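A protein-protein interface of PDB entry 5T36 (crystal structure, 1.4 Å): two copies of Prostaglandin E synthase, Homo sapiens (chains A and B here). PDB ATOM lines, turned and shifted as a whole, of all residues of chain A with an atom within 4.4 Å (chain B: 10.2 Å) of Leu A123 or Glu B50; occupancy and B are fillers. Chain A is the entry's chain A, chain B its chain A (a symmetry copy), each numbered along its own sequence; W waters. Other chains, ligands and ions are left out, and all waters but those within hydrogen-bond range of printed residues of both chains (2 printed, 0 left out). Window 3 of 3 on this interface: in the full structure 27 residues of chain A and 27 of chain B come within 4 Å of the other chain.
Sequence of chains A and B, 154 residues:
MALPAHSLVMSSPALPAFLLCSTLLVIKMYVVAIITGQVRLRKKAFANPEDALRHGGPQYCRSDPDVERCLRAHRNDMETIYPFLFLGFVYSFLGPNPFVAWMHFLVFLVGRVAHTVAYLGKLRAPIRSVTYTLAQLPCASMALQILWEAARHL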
ATOM      1  N   ARG A  69      20.044 -25.378  25.527  1.00  0.00           N
ATOM      2  CA  ARG A  69      20.860 -24.489  26.356  1.00  0.00           C
ATOM      3  C   ARG A  69      22.076 -25.222  26.931  1.00  0.00           C
ATOM      4  O   ARG A  69      23.195 -24.705  26.886  1.00  0.00           O
ATOM      5  CB  ARG A  69      20.014 -23.882  27.479  1.00  0.00           C
ATOM      6  CG  ARG A  69      20.770 -22.932  28.404  1.00  0.00           C
ATOM      7  CD  ARG A  69      19.831 -22.260  29.394  1.00  0.00           C
ATOM      8  NE  ARG A  69      18.936 -21.312  28.734  1.00  0.00           N
ATOM      9  CZ  ARG A  69      19.211 -20.026  28.535  1.00  0.00           C
ATOM     10  NH1 ARG A  69      20.361 -19.509  28.950  1.00  0.00           N
ATOM     11  NH2 ARG A  69      18.329 -19.250  27.920  1.00  0.00           N
ATOM     12  N   ALA A 118      26.259 -18.631  34.671  1.00  0.00           N
ATOM     13  CA  ALA A 118      25.489 -17.600  33.972  1.00  0.00           C
ATOM     14  C   ALA A 118      24.661 -18.162  32.817  1.00  0.00           C
ATOM     15  O   ALA A 118      23.557 -17.678  32.550  1.00  0.00           O
ATOM     16  CB  ALA A 118      26.406 -16.490  33.477  1.00  0.00           C
ATOM     17  N   GLY A 121      22.102 -20.994  34.449  1.00  0.00           N
ATOM     18  CA  GLY A 121      21.249 -20.269  35.391  1.00  0.00           C
ATOM     19  C   GLY A 121      20.413 -19.173  34.754  1.00  0.00           C
ATOM     20  O   GLY A 121      19.629 -18.512  35.440  1.00  0.00           O
ATOM     21  N   LYS A 122      20.590 -18.983  33.444  1.00  0.00           N
ATOM     22  CA  LYS A 122      19.826 -18.008  32.651  1.00  0.00           C
ATOM     23  C   LYS A 122      19.905 -16.583  33.213  1.00  0.00           C
ATOM     24  O   LYS A 122      18.903 -15.862  33.256  1.00  0.00           O
ATOM     25  CB  LYS A 122      18.361 -18.453  32.494  1.00  0.00           C
ATOM     26  CG  LYS A 122      18.184 -19.859  31.938  1.00  0.00           C
ATOM     27  CD  LYS A 122      16.730 -20.298  31.982  1.00  0.00           C
ATOM     28  CE  LYS A 122      16.588 -21.759  31.588  1.00  0.00           C
ATOM     29  NZ  LYS A 122      15.184 -22.236  31.712  1.00  0.00           N
ATOM     30  N   LEU A 123      21.101 -16.187  33.641  1.00  0.00           N
ATOM     31  CA  LEU A 123      21.317 -14.851  34.194  1.00  0.00           C
ATOM     32  C   LEU A 123      21.222 -13.787  33.104  1.00  0.00           C
ATOM     33  O   LEU A 123      21.512 -14.056  31.935  1.00  0.00           O
ATOM     34  CB  LEU A 123      22.661 -14.765  34.929  1.00  0.00           C
ATOM     35  CG  LEU A 123      22.876 -15.640  36.172  1.00  0.00           C
ATOM     36  CD1 LEU A 123      24.247 -15.373  36.775  1.00  0.00           C
ATOM     37  CD2 LEU A 123      21.788 -15.432  37.223  1.00  0.00           C
ATOM     38  N   ARG A 124      20.804 -12.585  33.494  1.00  0.00           N
ATOM     39  CA  ARG A 124      20.576 -11.492  32.547  1.00  0.00           C
ATOM     40  C   ARG A 124      21.839 -11.105  31.775  1.00  0.00           C
ATOM     41  O   ARG A 124      22.956 -11.230  32.283  1.00  0.00           O
ATOM     42  CB  ARG A 124      19.987 -10.267  33.262  1.00  0.00           C
ATOM     43  CG  ARG A 124      20.942  -9.573  34.227  1.00  0.00           C
ATOM     44  CD  ARG A 124      20.275  -8.417  34.950  1.00  0.00           C
ATOM     45  NE  ARG A 124      21.232  -7.655  35.752  1.00  0.00           N
ATOM     46  CZ  ARG A 124      21.584  -7.952  37.002  1.00  0.00           C
ATOM     47  NH1 ARG A 124      21.062  -9.006  37.619  1.00  0.00           N
ATOM     48  NH2 ARG A 124      22.465  -7.192  37.638  1.00  0.00           N
ATOM     49  N   ALA A 125      21.647 -10.654  30.539  1.00  0.00           N
ATOM     50  CA  ALA A 125      22.735 -10.117  29.733  1.00  0.00           C
ATOM     51  C   ALA A 125      23.192  -8.778  30.320  1.00  0.00           C
ATOM     52  O   ALA A 125      22.376  -8.043  30.881  1.00  0.00           O
ATOM     53  CB  ALA A 125      22.287  -9.950  28.289  1.00  0.00           C
ATOM     54  N   ILE A 127      25.909 -10.567  31.501  1.00  0.00           N
ATOM     55  CA  ILE A 127      26.721 -11.304  32.486  1.00  0.00           C
ATOM     56  C   ILE A 127      27.529 -12.441  31.847  1.00  0.00           C
ATOM     57  O   ILE A 127      28.747 -12.508  32.020  1.00  0.00           O
ATOM     58  CB  ILE A 127      25.882 -11.806  33.697  1.00  0.00           C
ATOM     59  CG1 ILE A 127      25.342 -10.613  34.498  1.00  0.00           C
ATOM     60  CG2 ILE A 127      26.716 -12.718  34.605  1.00  0.00           C
ATOM     61  CD1 ILE A 127      24.250 -10.964  35.499  1.00  0.00           C
ATOM     62  N   ARG A 128      26.857 -13.316  31.099  1.00  0.00           N
ATOM     63  CA  ARG A 128      27.533 -14.434  30.432  1.00  0.00           C
ATOM     64  C   ARG A 128      28.602 -13.948  29.450  1.00  0.00           C
ATOM     65  O   ARG A 128      29.720 -14.468  29.437  1.00  0.00           O
ATOM     66  CB  ARG A 128      26.525 -15.340  29.716  1.00  0.00           C
ATOM     67  CG  ARG A 128      27.132 -16.623  29.162  1.00  0.00           C
ATOM     68  CD  ARG A 128      26.264 -17.242  28.083  1.00  0.00           C
ATOM     69  NE  ARG A 128      26.302 -16.492  26.827  1.00  0.00           N
ATOM     70  CZ  ARG A 128      25.308 -15.740  26.360  1.00  0.00           C
ATOM     71  NH1 ARG A 128      24.168 -15.629  27.034  1.00  0.00           N
ATOM     72  NH2 ARG A 128      25.452 -15.103  25.206  1.00  0.00           N
ATOM     73  N   LEU B  41      25.076  -9.731  16.454  1.00  0.00           N
ATOM     74  CA  LEU B  41      24.669  -8.360  16.767  1.00  0.00           C
ATOM     75  C   LEU B  41      24.137  -7.612  15.545  1.00  0.00           C
ATOM     76  O   LEU B  41      23.103  -6.944  15.623  1.00  0.00           O
ATOM     77  CB  LEU B  41      25.833  -7.580  17.389  1.00  0.00           C
ATOM     78  CG  LEU B  41      26.244  -7.902  18.829  1.00  0.00           C
ATOM     79  CD1 LEU B  41      27.623  -7.330  19.121  1.00  0.00           C
ATOM     80  CD2 LEU B  41      25.221  -7.382  19.833  1.00  0.00           C
ATOM     81  N   PHE B  46      20.045 -14.005  17.970  1.00  0.00           N
ATOM     82  CA  PHE B  46      20.626 -14.511  19.204  1.00  0.00           C
ATOM     83  C   PHE B  46      20.065 -15.885  19.539  1.00  0.00           C
ATOM     84  O   PHE B  46      18.932 -16.209  19.176  1.00  0.00           O
ATOM     85  CB  PHE B  46      20.382 -13.514  20.341  1.00  0.00           C
ATOM     86  CG  PHE B  46      20.806 -12.110  20.006  1.00  0.00           C
ATOM     87  CD1 PHE B  46      22.138 -11.724  20.130  1.00  0.00           C
ATOM     88  CD2 PHE B  46      19.879 -11.182  19.542  1.00  0.00           C
ATOM     89  CE1 PHE B  46      22.539 -10.431  19.809  1.00  0.00           C
ATOM     90  CE2 PHE B  46      20.270  -9.888  19.217  1.00  0.00           C
ATOM     91  CZ  PHE B  46      21.604  -9.511  19.351  1.00  0.00           C
ATOM     92  N   ALA B  47      20.875 -16.692  20.216  1.00  0.00           N
ATOM     93  CA  ALA B  47      20.496 -18.055  20.566  1.00  0.00           C
ATOM     94  C   ALA B  47      19.759 -18.120  21.902  1.00  0.00           C
ATOM     95  O   ALA B  47      19.139 -19.136  22.228  1.00  0.00           O
ATOM     96  CB  ALA B  47      21.726 -18.946  20.595  1.00  0.00           C
ATOM     97  N   ASN B  48      19.820 -17.027  22.659  1.00  0.00           N
ATOM     98  CA  ASN B  48      19.271 -16.982  24.011  1.00  0.00           C
ATOM     99  C   ASN B  48      18.277 -15.842  24.200  1.00  0.00           C
ATOM    100  O   ASN B  48      18.536 -14.720  23.755  1.00  0.00           O
ATOM    101  CB  ASN B  48      20.403 -16.845  25.028  1.00  0.00           C
ATOM    102  CG  ASN B  48      21.429 -17.950  24.908  1.00  0.00           C
ATOM    103  OD1 ASN B  48      21.120 -19.120  25.121  1.00  0.00           O
ATOM    104  ND2 ASN B  48      22.657 -17.584  24.562  1.00  0.00           N
ATOM    105  N   PRO B  49      17.138 -16.122  24.867  1.00  0.00           N
ATOM    106  CA  PRO B  49      16.135 -15.087  25.137  1.00  0.00           C
ATOM    107  C   PRO B  49      16.688 -13.906  25.935  1.00  0.00           C
ATOM    108  O   PRO B  49      16.287 -12.766  25.689  1.00  0.00           O
ATOM    109  CB  PRO B  49      15.074 -15.830  25.955  1.00  0.00           C
ATOM    110  CG  PRO B  49      15.211 -17.245  25.546  1.00  0.00           C
ATOM    111  CD  PRO B  49      16.678 -17.450  25.313  1.00  0.00           C
ATOM    112  N   GLU B  50      17.602 -14.169  26.870  1.00  0.00           N
ATOM    113  CA  GLU B  50      18.198 -13.098  27.676  1.00  0.00           C
ATOM    114  C   GLU B  50      19.056 -12.143  26.840  1.00  0.00           C
ATOM    115  O   GLU B  50      19.112 -10.945  27.124  1.00  0.00           O
ATOM    116  CB  GLU B  50      18.981 -13.650  28.882  1.00  0.00           C
ATOM    117  CG  GLU B  50      20.211 -14.505  28.551  1.00  0.00           C
ATOM    118  CD  GLU B  50      19.912 -15.994  28.443  1.00  0.00           C
ATOM    119  OE1 GLU B  50      18.773 -16.373  28.092  1.00  0.00           O
ATOM    120  OE2 GLU B  50      20.838 -16.793  28.700  1.00  0.00           O
ATOM    121  N   ASP B  51      19.709 -12.679  25.809  1.00  0.00           N
ATOM    122  CA  ASP B  51      20.481 -11.871  24.867  1.00  0.00           C
ATOM    123  C   ASP B  51      19.543 -11.008  24.023  1.00  0.00           C
ATOM    124  O   ASP B  51      19.768  -9.807  23.862  1.00  0.00           O
ATOM    125  CB  ASP B  51      21.332 -12.757  23.945  1.00  0.00           C
ATOM    126  CG  ASP B  51      22.263 -13.698  24.705  1.00  0.00           C
ATOM    127  OD1 ASP B  51      22.438 -13.544  25.930  1.00  0.00           O
ATOM    128  OD2 ASP B  51      22.827 -14.605  24.057  1.00  0.00           O
ATOM    129  N   ALA B  52      18.487 -11.636  23.505  1.00  0.00           N
ATOM    130  CA  ALA B  52      17.520 -10.978  22.625  1.00  0.00           C
ATOM    131  C   ALA B  52      16.795  -9.811  23.294  1.00  0.00           C
ATOM    132  O   ALA B  52      16.621  -8.753  22.682  1.00  0.00           O
ATOM    133  CB  ALA B  52      16.519 -11.992  22.093  1.00  0.00           C
ATOM    134  N   LEU B  53      16.388 -10.002  24.548  1.00  0.00           N
ATOM    135  CA  LEU B  53      15.676  -8.966  25.304  1.00  0.00           C
ATOM    136  C   LEU B  53      16.542  -7.735  25.567  1.00  0.00           C
ATOM    137  O   LEU B  53      16.029  -6.622  25.688  1.00  0.00           O
ATOM    138  CB  LEU B  53      15.125  -9.525  26.621  1.00  0.00           C
ATOM    139  CG  LEU B  53      13.948 -10.508  26.555  1.00  0.00           C
ATOM    140  CD1 LEU B  53      13.734 -11.189  27.901  1.00  0.00           C
ATOM    141  CD2 LEU B  53      12.665  -9.826  26.092  1.00  0.00           C
ATOM    142  N   ARG B  54      17.854  -7.944  25.652  1.00  0.00           N
ATOM    143  CA  ARG B  54      18.813  -6.859  25.831  1.00  0.00           C
ATOM    144  C   ARG B  54      19.026  -6.088  24.525  1.00  0.00           C
ATOM    145  O   ARG B  54      19.325  -4.892  24.546  1.00  0.00           O
ATOM    146  CB  ARG B  54      20.143  -7.419  26.352  1.00  0.00           C
ATOM    147  CG  ARG B  54      21.055  -6.410  27.049  1.00  0.00           C
ATOM    148  CD  ARG B  54      22.152  -5.902  26.128  1.00  0.00           C
ATOM    149  NE  ARG B  54      23.246  -5.275  26.868  1.00  0.00           N
ATOM    150  CZ  ARG B  54      23.385  -3.964  27.049  1.00  0.00           C
ATOM    151  NH1 ARG B  54      22.500  -3.114  26.541  1.00  0.00           N
ATOM    152  NH2 ARG B  54      24.419  -3.499  27.738  1.00  0.00           N
ATOM    153  N   HIS B  55      18.855  -6.773  23.394  1.00  0.00           N
ATOM    154  CA  HIS B  55      19.172  -6.198  22.088  1.00  0.00           C
ATOM    155  C   HIS B  55      17.977  -6.047  21.139  1.00  0.00           C
ATOM    156  O   HIS B  55      18.097  -6.299  19.937  1.00  0.00           O
ATOM    157  CB  HIS B  55      20.282  -7.006  21.408  1.00  0.00           C
ATOM    158  CG  HIS B  55      21.590  -6.965  22.131  1.00  0.00           C
ATOM    159  ND1 HIS B  55      22.466  -5.908  22.023  1.00  0.00           N
ATOM    160  CD2 HIS B  55      22.175  -7.855  22.967  1.00  0.00           C
ATOM    161  CE1 HIS B  55      23.533  -6.144  22.766  1.00  0.00           C
ATOM    162  NE2 HIS B  55      23.382  -7.321  23.348  1.00  0.00           N
ATOM    163  N   GLY B  56      16.830  -5.632  21.672  1.00  0.00           N
ATOM    164  CA  GLY B  56      15.690  -5.280  20.826  1.00  0.00           C
ATOM    165  C   GLY B  56      14.355  -5.924  21.147  1.00  0.00           C
ATOM    166  O   GLY B  56      13.305  -5.346  20.864  1.00  0.00           O
ATOM    167  N   GLY B  57      14.388  -7.122  21.724  1.00  0.00           N
ATOM    168  CA  GLY B  57      13.163  -7.843  22.069  1.00  0.00           C
ATOM    169  C   GLY B  57      13.220  -9.332  21.773  1.00  0.00           C
ATOM    170  O   GLY B  57      14.172  -9.802  21.148  1.00  0.00           O
ATOM    171  N   PRO B  58      12.184 -10.080  22.205  1.00  0.00           N
ATOM    172  CA  PRO B  58      12.141 -11.546  22.127  1.00  0.00           C
ATOM    173  C   PRO B  58      12.135 -12.104  20.703  1.00  0.00           C
ATOM    174  O   PRO B  58      12.530 -13.254  20.495  1.00  0.00           O
ATOM    175  CB  PRO B  58      10.828 -11.897  22.835  1.00  0.00           C
ATOM    176  CG  PRO B  58       9.986 -10.682  22.698  1.00  0.00           C
ATOM    177  CD  PRO B  58      10.936  -9.529  22.767  1.00  0.00           C
ATOM    178  N   GLN B  59      11.698 -11.295  19.738  1.00  0.00           N
ATOM    179  CA  GLN B  59      11.660 -11.695  18.329  1.00  0.00           C
ATOM    180  C   GLN B  59      13.059 -11.910  17.740  1.00  0.00           C
ATOM    181  O   GLN B  59      13.204 -12.541  16.689  1.00  0.00           O
ATOM    182  CB  GLN B  59      10.871 -10.681  17.486  1.00  0.00           C
ATOM    183  CG  GLN B  59      11.545  -9.315  17.291  1.00  0.00           C
ATOM    184  CD  GLN B  59      11.008  -8.233  18.218  1.00  0.00           C
ATOM    185  OE1 GLN B  59      10.662  -7.141  17.768  1.00  0.00           O
ATOM    186  NE2 GLN B  59      10.936  -8.528  19.510  1.00  0.00           N
ATOM    187  N   TYR B  60      14.076 -11.390  18.424  1.00  0.00           N
ATOM    188  CA  TYR B  60      15.457 -11.505  17.958  1.00  0.00           C
ATOM    189  C   TYR B  60      16.179 -12.753  18.480  1.00  0.00           C
ATOM    190  O   TYR B  60      17.356 -12.967  18.174  1.00  0.00           O
ATOM    191  CB  TYR B  60      16.242 -10.221  18.247  1.00  0.00           C
ATOM    192  CG  TYR B  60      15.664  -9.009  17.549  1.00  0.00           C
ATOM    193  CD1 TYR B  60      15.615  -8.941  16.155  1.00  0.00           C
ATOM    194  CD2 TYR B  60      15.160  -7.934  18.278  1.00  0.00           C
ATOM    195  CE1 TYR B  60      15.082  -7.833  15.505  1.00  0.00           C
ATOM    196  CE2 TYR B  60      14.624  -6.820  17.638  1.00  0.00           C
ATOM    197  CZ  TYR B  60      14.590  -6.778  16.254  1.00  0.00           C
ATOM    198  OH  TYR B  60      14.063  -5.680  15.613  1.00  0.00           O
ATOM    199  N   CYS B  61      15.472 -13.565  19.266  1.00  0.00           N
ATOM    200  CA  CYS B  61      15.941 -14.912  19.580  1.00  0.00           C
ATOM    201  C   CYS B  61      15.530 -15.797  18.410  1.00  0.00           C
ATOM    202  O   CYS B  61      14.426 -16.349  18.381  1.00  0.00           O
ATOM    203  CB  CYS B  61      15.365 -15.426  20.902  1.00  0.00           C
ATOM    204  SG  CYS B  61      16.130 -16.968  21.479  1.00  0.00           S
ATOM    205  N   ARG B  62      16.427 -15.895  17.433  1.00  0.00           N
ATOM    206  CA  ARG B  62      16.128 -16.521  16.150  1.00  0.00           C
ATOM    207  C   ARG B  62      17.405 -17.016  15.479  1.00  0.00           C
ATOM    208  O   ARG B  62      18.506 -16.569  15.815  1.00  0.00           O
ATOM    209  CB  ARG B  62      15.410 -15.523  15.230  1.00  0.00           C
ATOM    210  CG  ARG B  62      16.217 -14.265  14.926  1.00  0.00           C
ATOM    211  CD  ARG B  62      15.452 -13.291  14.051  1.00  0.00           C
ATOM    212  NE  ARG B  62      16.243 -12.090  13.787  1.00  0.00           N
ATOM    213  CZ  ARG B  62      15.867 -11.091  12.993  1.00  0.00           C
ATOM    214  NH1 ARG B  62      14.696 -11.130  12.367  1.00  0.00           N
ATOM    215  NH2 ARG B  62      16.667 -10.047  12.826  1.00  0.00           N
HETATM  216  O   HOH W   1      18.891 -10.171  29.685  1.00  0.00           O
HETATM  217  O   HOH W   2      23.265 -16.423  29.898  1.00  0.00           O
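OE2 of Glu B50 lies within salt-bridge range of NH1 of Arg A69 (2.8 Å).
The guanidinium group (NH1) of Arg A128 lies close to the side-chain amide nitrogen (ND2) of Asn B48, 3.5 Å away.
NH1 of Arg A128 is in salt-bridge range of OE2 of Glu B50 (3.9 Å).
The side-chain carboxylate (OD2) of Asp B51 lies within salt-bridge range of the guanidinium group (NH2) of Arg A128, 2.9 Å away.
O of Ala A118 lies within hydrogen-bond range of N of Leu A123 (3.1 Å).
The side-chain amide nitrogen of Asn B48 sits at hydrogen-bond distance from the side-chain carboxylate of Asp B51, at 3.0 Å.
Water W1 lies within hydrogen-bond range of the backbone carbonyl oxygen of Glu B50 (2.7 Å) and the backbone NH of Ala A125 (2.9 Å).
Water W2 lies within hydrogen-bond range of the side-chain carboxylate of Glu B50, the backbone carbonyl oxygen of Ala A118 and the guanidinium group of Arg A128.
Of chain A, only Arg A69 (2.8 Å), Leu A123 (3.7 Å), Ala A125 (3.5 Å) and Arg A128 (3.9 Å) come within 4 Å of Glu B50.
Ala A125 touches just these residues of chain B: Glu B50 (3.5 Å) and Arg B54 (3.8 Å).
Printed residues of chain A within 4 Å of Asn B48: Arg A69 and Arg A128.
Of the printed residues of chain B, Arg A128 touches Asn B48, Glu B50 and Asp B51.
Printed residues of chain A within 4 Å of Pro B49: Arg A69 (3.6 Å).
Of the printed residues of chain B, Arg A69 touches Asn B48, Pro B49 and Glu B50.
Of the printed residues of chain A, Asp B51 touches Arg A128.
The nearest residue of chain B that does not touch Leu A123 is Asp B51 (6.1 Å).
The nearest printed residue of chain A that does not touch Pro B49 is Ala A125 (7.1 Å).
Of the 9 printed residues of chain A, 4 touch a printed residue of chain B.
Hydrophobic or aromatic side chains of chain A within 4 Å of the printed part of chain B: Ala A125.
Of the 18 printed residues of chain B, 5 touch a printed residue of chain A.
Hydrophobic or aromatic side chains of chain B within 4 Å of the printed part of chain A: Pro B49.
Among the printed residues, 9 pairs touch across the chains.
Among the printed residues, pairs that only touch across the chains: Ala A125 with Glu B50, Arg A69 with Pro B49, Leu A123 with Glu B50, Ala A125 with Arg B54 and Arg A69 with Asn B48.
No position is printed for both chains.
Of the 9 pairs that touch across the chains among the printed residues, none has its exchanged pair printed and touching as well.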
